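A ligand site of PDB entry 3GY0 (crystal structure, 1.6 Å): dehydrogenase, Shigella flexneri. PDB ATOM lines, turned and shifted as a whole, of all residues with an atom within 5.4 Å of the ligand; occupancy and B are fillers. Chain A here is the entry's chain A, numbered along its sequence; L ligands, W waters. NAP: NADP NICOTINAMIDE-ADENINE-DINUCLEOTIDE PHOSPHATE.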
ATOM      1  N   GLY A  17     -17.705  25.762  -9.851  1.00  0.00           N
ATOM      2  CA  GLY A  17     -16.604  24.938  -9.409  1.00  0.00           C
ATOM      3  C   GLY A  17     -15.339  25.805  -9.321  1.00  0.00           C
ATOM      4  O   GLY A  17     -14.249  25.327  -9.617  1.00  0.00           O
ATOM      5  N   ALA A  18     -15.497  27.063  -8.899  1.00  0.00           N
ATOM      6  CA  ALA A  18     -14.354  28.003  -8.837  1.00  0.00           C
ATOM      7  C   ALA A  18     -13.509  27.810  -7.573  1.00  0.00           C
ATOM      8  O   ALA A  18     -12.471  28.468  -7.391  1.00  0.00           O
ATOM      9  CB  ALA A  18     -14.884  29.444  -8.906  1.00  0.00           C
ATOM     10  N   SER A  19     -13.973  26.919  -6.690  1.00  0.00           N
ATOM     11  CA  SER A  19     -13.303  26.686  -5.410  1.00  0.00           C
ATOM     12  C   SER A  19     -12.111  25.722  -5.488  1.00  0.00           C
ATOM     13  O   SER A  19     -11.323  25.651  -4.545  1.00  0.00           O
ATOM     14  CB  SER A  19     -14.328  26.227  -4.367  1.00  0.00           C
ATOM     15  OG  SER A  19     -15.246  25.297  -4.930  1.00  0.00           O
ATOM     16  N   ASP A  20     -11.957  24.988  -6.605  1.00  0.00           N
ATOM     17  CA  ASP A  20     -10.858  24.031  -6.701  1.00  0.00           C
ATOM     18  C   ASP A  20     -10.483  23.717  -8.142  1.00  0.00           C
ATOM     19  O   ASP A  20     -11.220  24.041  -9.060  1.00  0.00           O
ATOM     20  CB  ASP A  20     -11.239  22.718  -6.002  1.00  0.00           C
ATOM     21  CG  ASP A  20     -10.083  22.082  -5.279  1.00  0.00           C
ATOM     22  OD1 ASP A  20      -8.886  22.441  -5.575  1.00  0.00           O
ATOM     23  OD2 ASP A  20     -10.354  21.203  -4.405  1.00  0.00           O
ATOM     24  N   GLY A  21      -9.341  23.048  -8.323  1.00  0.00           N
ATOM     25  CA  GLY A  21      -9.027  22.411  -9.614  1.00  0.00           C
ATOM     26  C   GLY A  21      -9.072  23.352 -10.797  1.00  0.00           C
ATOM     27  O   GLY A  21      -8.541  24.470 -10.752  1.00  0.00           O
ATOM     28  N   ILE A  22      -9.694  22.897 -11.868  1.00  0.00           N
ATOM     29  CA  ILE A  22      -9.708  23.659 -13.128  1.00  0.00           C
ATOM     30  C   ILE A  22     -10.486  24.978 -12.978  1.00  0.00           C
ATOM     31  O   ILE A  22     -10.075  26.022 -13.508  1.00  0.00           O
ATOM     32  CB  ILE A  22     -10.292  22.801 -14.279  1.00  0.00           C
ATOM     33  CG1 ILE A  22      -9.393  21.569 -14.494  1.00  0.00           C
ATOM     34  CG2 ILE A  22     -10.427  23.626 -15.562  1.00  0.00           C
ATOM     35  CD1 ILE A  22     -10.009  20.504 -15.419  1.00  0.00           C
ATOM     36  N   GLY A  23     -11.626  24.923 -12.294  1.00  0.00           N
ATOM     37  CA  GLY A  23     -12.461  26.115 -12.132  1.00  0.00           C
ATOM     38  C   GLY A  23     -11.737  27.221 -11.374  1.00  0.00           C
ATOM     39  O   GLY A  23     -11.837  28.399 -11.736  1.00  0.00           O
ATOM     40  N   GLY A  41     -19.385  28.134  -5.874  1.00  0.00           N
ATOM     41  CA  GLY A  41     -18.944  26.845  -5.359  1.00  0.00           C
ATOM     42  C   GLY A  41     -19.846  26.379  -4.247  1.00  0.00           C
ATOM     43  O   GLY A  41     -20.924  26.940  -4.023  1.00  0.00           O
ATOM     44  N   ARG A  42     -19.386  25.372  -3.543  1.00  0.00           N
ATOM     45  CA  ARG A  42     -20.132  24.791  -2.451  1.00  0.00           C
ATOM     46  C   ARG A  42     -19.417  25.089  -1.118  1.00  0.00           C
ATOM     47  O   ARG A  42     -20.072  25.451  -0.123  1.00  0.00           O
ATOM     48  CB  ARG A  42     -20.252  23.282  -2.751  1.00  0.00           C
ATOM     49  CG  ARG A  42     -20.774  22.451  -1.669  1.00  0.00           C
ATOM     50  CD  ARG A  42     -20.973  21.032  -2.212  1.00  0.00           C
ATOM     51  NE  ARG A  42     -19.721  20.444  -2.711  1.00  0.00           N
ATOM     52  CZ  ARG A  42     -19.504  19.118  -2.787  1.00  0.00           C
ATOM     53  NH1 ARG A  42     -18.337  18.679  -3.242  1.00  0.00           N
ATOM     54  NH2 ARG A  42     -20.440  18.265  -2.400  1.00  0.00           N
ATOM     55  N   ASN A  43     -18.092  24.945  -1.115  1.00  0.00           N
ATOM     56  CA  ASN A  43     -17.266  25.117   0.084  1.00  0.00           C
ATOM     57  C   ASN A  43     -16.900  26.579   0.343  1.00  0.00           C
ATOM     58  O   ASN A  43     -16.066  27.173  -0.367  1.00  0.00           O
ATOM     59  CB  ASN A  43     -16.017  24.239  -0.010  1.00  0.00           C
ATOM     60  CG  ASN A  43     -15.259  24.163   1.292  1.00  0.00           C
ATOM     61  OD1 ASN A  43     -14.494  25.054   1.635  1.00  0.00           O
ATOM     62  ND2 ASN A  43     -15.490  23.091   2.064  1.00  0.00           N
ATOM     63  N   LYS A  46     -13.059  27.460   0.938  1.00  0.00           N
ATOM     64  CA  LYS A  46     -12.318  27.439  -0.320  1.00  0.00           C
ATOM     65  C   LYS A  46     -12.638  28.667  -1.165  1.00  0.00           C
ATOM     66  O   LYS A  46     -11.725  29.258  -1.744  1.00  0.00           O
ATOM     67  CB  LYS A  46     -12.581  26.157  -1.137  1.00  0.00           C
ATOM     68  CG  LYS A  46     -11.837  24.931  -0.578  1.00  0.00           C
ATOM     69  CD  LYS A  46     -12.075  23.693  -1.466  1.00  0.00           C
ATOM     70  CE  LYS A  46     -11.310  22.479  -0.910  1.00  0.00           C
ATOM     71  NZ  LYS A  46     -11.560  21.241  -1.721  1.00  0.00           N
ATOM     72  N   LEU A  67     -23.751  27.773  -3.979  1.00  0.00           N
ATOM     73  CA  LEU A  67     -24.885  27.085  -4.595  1.00  0.00           C
ATOM     74  C   LEU A  67     -24.545  25.622  -4.668  1.00  0.00           C
ATOM     75  O   LEU A  67     -23.671  25.224  -5.455  1.00  0.00           O
ATOM     76  CB  LEU A  67     -25.175  27.631  -5.999  1.00  0.00           C
ATOM     77  CG  LEU A  67     -26.428  27.098  -6.707  1.00  0.00           C
ATOM     78  CD1 LEU A  67     -27.694  27.577  -6.024  1.00  0.00           C
ATOM     79  CD2 LEU A  67     -26.393  27.524  -8.160  1.00  0.00           C
ATOM     80  N   ASP A  68     -25.221  24.806  -3.864  1.00  0.00           N
ATOM     81  CA  ASP A  68     -24.969  23.372  -3.868  1.00  0.00           C
ATOM     82  C   ASP A  68     -25.844  22.772  -4.961  1.00  0.00           C
ATOM     83  O   ASP A  68     -27.086  22.750  -4.837  1.00  0.00           O
ATOM     84  CB  ASP A  68     -25.293  22.744  -2.521  1.00  0.00           C
ATOM     85  CG  ASP A  68     -24.862  21.290  -2.461  1.00  0.00           C
ATOM     86  OD1 ASP A  68     -24.589  20.816  -1.333  1.00  0.00           O
ATOM     87  OD2 ASP A  68     -24.759  20.622  -3.503  1.00  0.00           O
ATOM     88  N   LEU A  69     -25.192  22.280  -6.010  1.00  0.00           N
ATOM     89  CA  LEU A  69     -25.873  21.799  -7.219  1.00  0.00           C
ATOM     90  C   LEU A  69     -26.616  20.493  -6.969  1.00  0.00           C
ATOM     91  O   LEU A  69     -27.470  20.094  -7.798  1.00  0.00           O
ATOM     92  CB  LEU A  69     -24.865  21.642  -8.370  1.00  0.00           C
ATOM     93  CG  LEU A  69     -24.258  22.974  -8.828  1.00  0.00           C
ATOM     94  CD1 LEU A  69     -23.095  22.728  -9.804  1.00  0.00           C
ATOM     95  CD2 LEU A  69     -25.307  23.865  -9.491  1.00  0.00           C
ATOM     96  N   LEU A  70     -26.287  19.808  -5.877  1.00  0.00           N
ATOM     97  CA  LEU A  70     -26.999  18.544  -5.572  1.00  0.00           C
ATOM     98  C   LEU A  70     -28.435  18.809  -5.110  1.00  0.00           C
ATOM     99  O   LEU A  70     -29.344  18.013  -5.376  1.00  0.00           O
ATOM    100  CB  LEU A  70     -26.250  17.722  -4.510  1.00  0.00           C
ATOM    101  CG  LEU A  70     -26.911  16.376  -4.183  1.00  0.00           C
ATOM    102  CD1 LEU A  70     -26.956  15.509  -5.427  1.00  0.00           C
ATOM    103  CD2 LEU A  70     -26.108  15.708  -3.079  1.00  0.00           C
ATOM    104  N   ASN A  97     -18.223  24.605 -14.966  1.00  0.00           N
ATOM    105  CA  ASN A  97     -17.089  23.725 -14.745  1.00  0.00           C
ATOM    106  C   ASN A  97     -17.373  22.748 -13.607  1.00  0.00           C
ATOM    107  O   ASN A  97     -16.768  21.668 -13.563  1.00  0.00           O
ATOM    108  CB  ASN A  97     -15.828  24.593 -14.489  1.00  0.00           C
ATOM    109  CG  ASN A  97     -14.778  23.847 -13.738  1.00  0.00           C
ATOM    110  OD1 ASN A  97     -13.913  23.190 -14.324  1.00  0.00           O
ATOM    111  ND2 ASN A  97     -14.824  23.950 -12.424  1.00  0.00           N
ATOM    112  N   ALA A  98     -18.252  23.094 -12.677  1.00  0.00           N
ATOM    113  CA  ALA A  98     -18.561  22.162 -11.558  1.00  0.00           C
ATOM    114  C   ALA A  98     -18.996  20.795 -12.103  1.00  0.00           C
ATOM    115  O   ALA A  98     -19.662  20.687 -13.127  1.00  0.00           O
ATOM    116  CB  ALA A  98     -19.676  22.755 -10.694  1.00  0.00           C
ATOM    117  N   GLY A  99     -18.599  19.751 -11.389  1.00  0.00           N
ATOM    118  CA  GLY A  99     -18.958  18.388 -11.826  1.00  0.00           C
ATOM    119  C   GLY A  99     -18.694  17.437 -10.687  1.00  0.00           C
ATOM    120  O   GLY A  99     -17.840  17.688  -9.828  1.00  0.00           O
ATOM    121  N   LEU A 100     -19.445  16.326 -10.710  1.00  0.00           N
ATOM    122  CA  LEU A 100     -19.226  15.207  -9.793  1.00  0.00           C
ATOM    123  C   LEU A 100     -18.802  14.014 -10.644  1.00  0.00           C
ATOM    124  O   LEU A 100     -19.418  13.725 -11.694  1.00  0.00           O
ATOM    125  CB  LEU A 100     -20.521  14.900  -9.036  1.00  0.00           C
ATOM    126  CG  LEU A 100     -20.401  13.732  -8.015  1.00  0.00           C
ATOM    127  CD1 LEU A 100     -19.464  14.106  -6.852  1.00  0.00           C
ATOM    128  CD2 LEU A 100     -21.786  13.357  -7.450  1.00  0.00           C
ATOM    129  N   ILE A 121     -26.239  16.907 -10.492  1.00  0.00           N
ATOM    130  CA  ILE A 121     -25.270  18.017 -10.515  1.00  0.00           C
ATOM    131  C   ILE A 121     -24.827  18.365 -11.934  1.00  0.00           C
ATOM    132  O   ILE A 121     -24.886  19.524 -12.328  1.00  0.00           O
ATOM    133  CB  ILE A 121     -24.031  17.634  -9.657  1.00  0.00           C
ATOM    134  CG1 ILE A 121     -24.461  17.580  -8.177  1.00  0.00           C
ATOM    135  CG2 ILE A 121     -22.829  18.602  -9.883  1.00  0.00           C
ATOM    136  CD1 ILE A 121     -23.503  16.729  -7.292  1.00  0.00           C
ATOM    137  N   THR A 148     -18.470  21.885 -19.633  1.00  0.00           N
ATOM    138  CA  THR A 148     -17.271  21.067 -19.534  1.00  0.00           C
ATOM    139  C   THR A 148     -17.604  19.611 -19.778  1.00  0.00           C
ATOM    140  O   THR A 148     -18.445  19.026 -19.078  1.00  0.00           O
ATOM    141  CB  THR A 148     -16.610  21.232 -18.165  1.00  0.00           C
ATOM    142  OG1 THR A 148     -16.436  22.631 -17.898  1.00  0.00           O
ATOM    143  CG2 THR A 148     -15.231  20.540 -18.126  1.00  0.00           C
ATOM    144  N   SER A 149     -16.963  19.032 -20.790  1.00  0.00           N
ATOM    145  CA  SER A 149     -17.201  17.654 -21.142  1.00  0.00           C
ATOM    146  C   SER A 149     -15.997  16.792 -20.706  1.00  0.00           C
ATOM    147  O   SER A 149     -15.247  17.159 -19.797  1.00  0.00           O
ATOM    148  CB  SER A 149     -17.512  17.544 -22.645  1.00  0.00           C
ATOM    149  OG  SER A 149     -17.992  16.224 -22.950  1.00  0.00           O
ATOM    150  N   SER A 150     -15.827  15.636 -21.356  1.00  0.00           N
ATOM    151  CA  SER A 150     -14.748  14.700 -21.055  1.00  0.00           C
ATOM    152  C   SER A 150     -14.634  13.834 -22.287  1.00  0.00           C
ATOM    153  O   SER A 150     -15.580  13.775 -23.073  1.00  0.00           O
ATOM    154  CB  SER A 150     -15.134  13.829 -19.868  1.00  0.00           C
ATOM    155  OG  SER A 150     -14.176  12.802 -19.677  1.00  0.00           O
ATOM    156  N   TYR A 163     -20.919   9.181 -14.913  1.00  0.00           N
ATOM    157  CA  TYR A 163     -20.125  10.272 -15.443  1.00  0.00           C
ATOM    158  C   TYR A 163     -20.177  10.332 -16.969  1.00  0.00           C
ATOM    159  O   TYR A 163     -20.458  11.412 -17.524  1.00  0.00           O
ATOM    160  CB  TYR A 163     -18.691  10.081 -14.987  1.00  0.00           C
ATOM    161  CG  TYR A 163     -17.762  11.229 -15.289  1.00  0.00           C
ATOM    162  CD1 TYR A 163     -17.828  12.411 -14.541  1.00  0.00           C
ATOM    163  CD2 TYR A 163     -16.775  11.104 -16.259  1.00  0.00           C
ATOM    164  CE1 TYR A 163     -16.935  13.442 -14.774  1.00  0.00           C
ATOM    165  CE2 TYR A 163     -15.870  12.148 -16.490  1.00  0.00           C
ATOM    166  CZ  TYR A 163     -15.969  13.305 -15.741  1.00  0.00           C
ATOM    167  OH  TYR A 163     -15.050  14.323 -15.951  1.00  0.00           O
ATOM    168  N   LYS A 167     -21.870  13.323 -19.175  1.00  0.00           N
ATOM    169  CA  LYS A 167     -21.083  14.168 -20.086  1.00  0.00           C
ATOM    170  C   LYS A 167     -21.642  14.058 -21.515  1.00  0.00           C
ATOM    171  O   LYS A 167     -21.575  15.029 -22.275  1.00  0.00           O
ATOM    172  CB  LYS A 167     -19.589  13.851 -20.005  1.00  0.00           C
ATOM    173  CG  LYS A 167     -18.966  14.168 -18.610  1.00  0.00           C
ATOM    174  CD  LYS A 167     -19.144  15.634 -18.208  1.00  0.00           C
ATOM    175  CE  LYS A 167     -18.207  15.957 -17.047  1.00  0.00           C
ATOM    176  NZ  LYS A 167     -18.272  17.416 -16.652  1.00  0.00           N
ATOM    177  N   ASN A 191     -13.413  19.985 -23.506  1.00  0.00           N
ATOM    178  CA  ASN A 191     -12.897  18.791 -22.878  1.00  0.00           C
ATOM    179  C   ASN A 191     -11.471  19.077 -22.422  1.00  0.00           C
ATOM    180  O   ASN A 191     -10.564  19.174 -23.260  1.00  0.00           O
ATOM    181  CB  ASN A 191     -12.910  17.620 -23.854  1.00  0.00           C
ATOM    182  CG  ASN A 191     -12.099  16.434 -23.355  1.00  0.00           C
ATOM    183  OD1 ASN A 191     -11.867  16.283 -22.139  1.00  0.00           O
ATOM    184  ND2 ASN A 191     -11.624  15.622 -24.291  1.00  0.00           N
ATOM    185  N   PRO A 192     -11.267  19.221 -21.098  1.00  0.00           N
ATOM    186  CA  PRO A 192      -9.938  19.559 -20.549  1.00  0.00           C
ATOM    187  C   PRO A 192      -8.870  18.527 -20.858  1.00  0.00           C
ATOM    188  O   PRO A 192      -7.711  18.887 -20.885  1.00  0.00           O
ATOM    189  CB  PRO A 192     -10.152  19.577 -19.034  1.00  0.00           C
ATOM    190  CG  PRO A 192     -11.629  19.609 -18.831  1.00  0.00           C
ATOM    191  CD  PRO A 192     -12.288  19.089 -20.044  1.00  0.00           C
ATOM    192  N   GLY A 193      -9.261  17.280 -21.088  1.00  0.00           N
ATOM    193  CA  GLY A 193      -8.298  16.184 -21.109  1.00  0.00           C
ATOM    194  C   GLY A 193      -7.858  15.840 -19.693  1.00  0.00           C
ATOM    195  O   GLY A 193      -8.236  16.497 -18.722  1.00  0.00           O
ATOM    196  N   GLY A 194      -7.031  14.809 -19.566  1.00  0.00           N
ATOM    197  CA  GLY A 194      -6.555  14.396 -18.251  1.00  0.00           C
ATOM    198  C   GLY A 194      -5.695  15.506 -17.656  1.00  0.00           C
ATOM    199  O   GLY A 194      -4.688  15.892 -18.248  1.00  0.00           O
ATOM    200  N   THR A 195      -6.110  15.991 -16.486  1.00  0.00           N
ATOM    201  CA  THR A 195      -5.550  17.209 -15.879  1.00  0.00           C
ATOM    202  C   THR A 195      -5.318  16.962 -14.396  1.00  0.00           C
ATOM    203  O   THR A 195      -6.102  16.275 -13.743  1.00  0.00           O
ATOM    204  CB  THR A 195      -6.500  18.426 -16.102  1.00  0.00           C
ATOM    205  OG1 THR A 195      -6.759  18.570 -17.500  1.00  0.00           O
ATOM    206  CG2 THR A 195      -5.846  19.732 -15.603  1.00  0.00           C
ATOM    207  N   ARG A 196      -4.221  17.512 -13.871  1.00  0.00           N
ATOM    208  CA  ARG A 196      -3.777  17.214 -12.503  1.00  0.00           C
ATOM    209  C   ARG A 196      -4.695  17.875 -11.461  1.00  0.00           C
ATOM    210  O   ARG A 196      -4.441  19.003 -11.020  1.00  0.00           O
ATOM    211  CB  ARG A 196      -2.312  17.649 -12.325  1.00  0.00           C
ATOM    212  CG  ARG A 196      -1.658  17.176 -11.008  1.00  0.00           C
ATOM    213  CD  ARG A 196      -0.205  17.668 -10.847  1.00  0.00           C
ATOM    214  NE  ARG A 196       0.609  17.470 -12.052  1.00  0.00           N
ATOM    215  CZ  ARG A 196       1.709  18.172 -12.351  1.00  0.00           C
ATOM    216  NH1 ARG A 196       2.139  19.129 -11.530  1.00  0.00           N
ATOM    217  NH2 ARG A 196       2.363  17.925 -13.476  1.00  0.00           N
ATOM    218  N   THR A 197      -5.756  17.169 -11.078  1.00  0.00           N
ATOM    219  CA  THR A 197      -6.693  17.595 -10.025  1.00  0.00           C
ATOM    220  C   THR A 197      -7.062  16.422  -9.139  1.00  0.00           C
ATOM    221  O   THR A 197      -6.720  15.263  -9.442  1.00  0.00           O
ATOM    222  CB  THR A 197      -8.018  18.139 -10.606  1.00  0.00           C
ATOM    223  OG1 THR A 197      -8.783  17.056 -11.157  1.00  0.00           O
ATOM    224  CG2 THR A 197      -7.774  19.163 -11.730  1.00  0.00           C
ATOM    225  N   ALA A 198      -7.814  16.702  -8.058  1.00  0.00           N
ATOM    226  CA  ALA A 198      -8.260  15.645  -7.139  1.00  0.00           C
ATOM    227  C   ALA A 198      -9.231  14.691  -7.831  1.00  0.00           C
ATOM    228  O   ALA A 198      -9.301  13.490  -7.481  1.00  0.00           O
ATOM    229  CB  ALA A 198      -8.932  16.251  -5.902  1.00  0.00           C
ATOM    230  N   MET A 199     -10.005  15.210  -8.779  1.00  0.00           N
ATOM    231  CA  MET A 199     -10.978  14.330  -9.450  1.00  0.00           C
ATOM    232  C   MET A 199     -10.245  13.271 -10.263  1.00  0.00           C
ATOM    233  O   MET A 199     -10.555  12.073 -10.198  1.00  0.00           O
ATOM    234  CB  MET A 199     -11.949  15.128 -10.340  1.00  0.00           C
ATOM    235  CG  MET A 199     -13.093  14.213 -10.891  1.00  0.00           C
ATOM    236  SD  MET A 199     -14.218  15.008 -12.115  1.00  0.00           S
ATOM    237  CE  MET A 199     -15.060  16.111 -11.033  1.00  0.00           C
ATOM    238  N   ARG A 200      -9.255  13.722 -11.035  1.00  0.00           N
ATOM    239  CA  ARG A 200      -8.444  12.844 -11.862  1.00  0.00           C
ATOM    240  C   ARG A 200      -7.694  11.821 -11.006  1.00  0.00           C
ATOM    241  O   ARG A 200      -7.638  10.641 -11.360  1.00  0.00           O
ATOM    242  CB  ARG A 200      -7.465  13.683 -12.684  1.00  0.00           C
ATOM    243  CG  ARG A 200      -6.524  12.877 -13.543  1.00  0.00           C
ATOM    244  CD  ARG A 200      -7.202  12.228 -14.719  1.00  0.00           C
ATOM    245  NE  ARG A 200      -6.240  11.373 -15.427  1.00  0.00           N
ATOM    246  CZ  ARG A 200      -6.408  10.901 -16.657  1.00  0.00           C
ATOM    247  NH1 ARG A 200      -7.500  11.212 -17.351  1.00  0.00           N
ATOM    248  NH2 ARG A 200      -5.471  10.118 -17.188  1.00  0.00           N
HETATM  249  PA  NAP L   1     -12.156  19.204  -8.742  1.00  0.00           P
HETATM  250  O1A NAP L   1     -10.871  19.861  -8.421  1.00  0.00           O
HETATM  251  O2A NAP L   1     -12.605  18.152  -7.787  1.00  0.00           O
HETATM  252  O5B NAP L   1     -13.250  20.367  -8.857  1.00  0.00           O
HETATM  253  C5B NAP L   1     -14.645  20.110  -8.984  1.00  0.00           C
HETATM  254  C4B NAP L   1     -15.377  21.400  -8.643  1.00  0.00           C
HETATM  255  O4B NAP L   1     -16.766  21.094  -8.763  1.00  0.00           O
HETATM  256  C3B NAP L   1     -15.092  21.852  -7.219  1.00  0.00           C
HETATM  257  O3B NAP L   1     -14.923  23.248  -7.195  1.00  0.00           O
HETATM  258  C2B NAP L   1     -16.422  21.561  -6.538  1.00  0.00           C
HETATM  259  O2B NAP L   1     -16.739  22.530  -5.562  1.00  0.00           O
HETATM  260  C1B NAP L   1     -17.443  21.625  -7.695  1.00  0.00           C
HETATM  261  N9A NAP L   1     -18.581  20.806  -7.255  1.00  0.00           N
HETATM  262  C8A NAP L   1     -18.594  19.428  -7.055  1.00  0.00           C
HETATM  263  N7A NAP L   1     -19.807  19.127  -6.549  1.00  0.00           N
HETATM  264  C5A NAP L   1     -20.543  20.268  -6.399  1.00  0.00           C
HETATM  265  C6A NAP L   1     -21.822  20.529  -5.888  1.00  0.00           C
HETATM  266  N6A NAP L   1     -22.618  19.583  -5.411  1.00  0.00           N
HETATM  267  N1A NAP L   1     -22.284  21.827  -5.874  1.00  0.00           N
HETATM  268  C2A NAP L   1     -21.492  22.867  -6.333  1.00  0.00           C
HETATM  269  N3A NAP L   1     -20.242  22.606  -6.815  1.00  0.00           N
HETATM  270  C4A NAP L   1     -19.766  21.329  -6.842  1.00  0.00           C
HETATM  271  O3  NAP L   1     -12.139  18.560 -10.198  1.00  0.00           O
HETATM  272  PN  NAP L   1     -11.746  19.142 -11.648  1.00  0.00           P
HETATM  273  O1N NAP L   1     -11.212  20.507 -11.503  1.00  0.00           O
HETATM  274  O2N NAP L   1     -10.916  18.096 -12.297  1.00  0.00           O
HETATM  275  O5D NAP L   1     -13.170  19.166 -12.370  1.00  0.00           O
HETATM  276  C5D NAP L   1     -13.628  20.314 -13.081  1.00  0.00           C
HETATM  277  C4D NAP L   1     -14.399  19.890 -14.319  1.00  0.00           C
HETATM  278  O4D NAP L   1     -13.462  19.302 -15.209  1.00  0.00           O
HETATM  279  C3D NAP L   1     -15.483  18.844 -14.017  1.00  0.00           C
HETATM  280  O3D NAP L   1     -16.647  19.172 -14.755  1.00  0.00           O
HETATM  281  C2D NAP L   1     -14.832  17.590 -14.553  1.00  0.00           C
HETATM  282  O2D NAP L   1     -15.821  16.660 -14.980  1.00  0.00           O
HETATM  283  C1D NAP L   1     -14.047  18.135 -15.719  1.00  0.00           C
HETATM  284  N1N NAP L   1     -12.987  17.264 -16.187  1.00  0.00           N
HETATM  285  C2N NAP L   1     -11.861  17.057 -15.428  1.00  0.00           C
HETATM  286  C3N NAP L   1     -10.848  16.239 -15.914  1.00  0.00           C
HETATM  287  C7N NAP L   1      -9.566  16.079 -15.163  1.00  0.00           C
HETATM  288  O7N NAP L   1      -8.666  15.192 -15.686  1.00  0.00           O
HETATM  289  N7N NAP L   1      -9.308  16.744 -14.026  1.00  0.00           N
HETATM  290  C4N NAP L   1     -10.979  15.633 -17.185  1.00  0.00           C
HETATM  291  C5N NAP L   1     -12.133  15.859 -17.931  1.00  0.00           C
HETATM  292  C6N NAP L   1     -13.144  16.680 -17.423  1.00  0.00           C
HETATM  293  P2B NAP L   1     -16.423  22.420  -3.968  1.00  0.00           P
HETATM  294  O1X NAP L   1     -16.757  23.796  -3.421  1.00  0.00           O
HETATM  295  O2X NAP L   1     -17.209  21.284  -3.328  1.00  0.00           O
HETATM  296  O3X NAP L   1     -14.959  22.113  -3.860  1.00  0.00           O
HETATM  297  O   HOH W   1     -11.987  18.909  -5.242  1.00  0.00           O
HETATM  298  O   HOH W   2     -12.837  22.690 -10.821  1.00  0.00           O
HETATM  299  O   HOH W   3     -19.920  25.187  -8.154  1.00  0.00           O
HETATM  300  O   HOH W   4     -13.989  19.823  -3.402  1.00  0.00           O
HETATM  301  O   HOH W   5     -20.912  16.899  -5.210  1.00  0.00           O
HETATM  302  O   HOH W   6      -8.576  19.343  -7.249  1.00  0.00           O
HETATM  303  O   HOH W   7     -16.326  20.660  -0.782  1.00  0.00           O
HETATM  304  O   HOH W   8     -15.122  18.304  -6.157  1.00  0.00           O
HETATM  305  O   HOH W   9     -16.692  16.623  -7.548  1.00  0.00           O
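The backbone carbonyl oxygen (O) of Gly 193 sits close to an oxygen (O7N) of the ligand, 3.3 Å away. Gly 21 touches the ligand (CA to O1A, 3.4 Å). Leu 67 touches the ligand (O to C2A, 3.3 Å). Leu 70 touches the ligand (N to N6A, 3.7 Å). CA of Ala 98 touches O4B of the ligand, at 3.5 Å. CD1 of Ile 121 touches N6A of the ligand (3.5 Å). Thr 148 touches the ligand (CG2 to C1D, 3.6 Å). Ser 149 touches the ligand (O to C6N, 3.2 Å). CG of Pro 192 touches C6N of the ligand (3.6 Å). Gly 194 touches the ligand (CA to O7N, 3.4 Å). CD of Arg 200 touches O7N of the ligand, at 3.4 Å. Hydrophobic or aromatic side chains that line the ligand: Ile 22, Leu 69, Ala 98, Ile 121, Tyr 163, Pro 192 and Met 199.
The backbone NH of Leu 70 is in hydrogen-bond range of the side-chain carboxylate of Asp 68, at 2.9 Å. The side-chain amide oxygen (OD1) of Asn 43 lies within hydrogen-bond range of the backbone NH (N) of Lys 46 (2.9 Å). The side-chain hydroxyl (OG1) of Thr 197 sits at hydrogen-bond distance from the backbone NH (N) of Arg 200, 3.4 Å away. NZ of Lys 167 sits at hydrogen-bond distance from O of Thr 148 (2.9 Å). The backbone carbonyl oxygen of Gly 193 sits at hydrogen-bond distance from the side-chain hydroxyl of Thr 195, at 2.8 Å. The backbone carbonyl oxygen of Gly 17 sits at hydrogen-bond distance from the side-chain amide nitrogen of Asn 97, 3.2 Å away. The backbone NH of Gly 193 lies within hydrogen-bond range of the side-chain amide oxygen of Asn 191 (3.0 Å). The backbone NH of Leu 67 lies within hydrogen-bond range of the backbone carbonyl oxygen of Gly 41 (2.9 Å).
Water W4 bridges an oxygen (O3X) of the ligand and the side-chain amino group of Lys 46. Water W6 lies within hydrogen-bond range of an oxygen (O1A) of the ligand (2.6 Å) and the backbone NH of Ala 198 (2.9 Å). Water W1 bridges O2A of the ligand (2.7 Å) and OD2 of Asp 20 (2.9 Å). Water W5 bridges N7A of the ligand (2.8 Å) and NH2 of Arg 42 (3.2 Å). Water W3 lies within hydrogen-bond range of N of Gly 17 (2.8 Å) and N3A of the ligand (2.9 Å).
The backbone NH (N) of Asn 43 lies within hydrogen-bond range of an oxygen (O1X) of the ligand, 2.9 Å away. N of Arg 42 sits at hydrogen-bond distance from O1X of the ligand (3.1 Å). N of Leu 69 lies within hydrogen-bond range of N1A of the ligand (2.9 Å). A nitrogen (N7N) of the ligand lies within hydrogen-bond range of the backbone carbonyl oxygen of Thr 195 (3.3 Å). N of Asp 20 sits at hydrogen-bond distance from O3B of the ligand (3.5 Å). The side-chain carboxylate (OD2) of Asp 68 sits at hydrogen-bond distance from a nitrogen (N6A) of the ligand (3.1 Å). The backbone carbonyl oxygen (O) of Gly 17 sits close to an oxygen (O3B) of the ligand (3.3 Å). OG1 of Thr 197 lies within hydrogen-bond range of O2N of the ligand (2.6 Å). The guanidinium group (NE) of Arg 42 is in salt-bridge range of an oxygen (O2X) of the ligand, at 2.7 Å. O2D of the ligand lies close to SD of Met 199 (3.7 Å). N of Gly 99 lies within hydrogen-bond range of O4B of the ligand, 3.5 Å away. The side-chain hydroxyl of Tyr 163 sits at hydrogen-bond distance from an oxygen (O2D) of the ligand (2.6 Å). NZ of Lys 167 is in hydrogen-bond range of O3D of the ligand (3.1 Å). The backbone NH (N) of Ile 22 sits at hydrogen-bond distance from an oxygen (O1N) of the ligand, 2.9 Å away. O7N of the ligand sits at hydrogen-bond distance from N of Thr 195 (2.8 Å). O of Asn 97 sits at hydrogen-bond distance from O3D of the ligand, 2.8 Å away. O1X of the ligand is in hydrogen-bond range of OG of Ser 19, at 2.6 Å.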
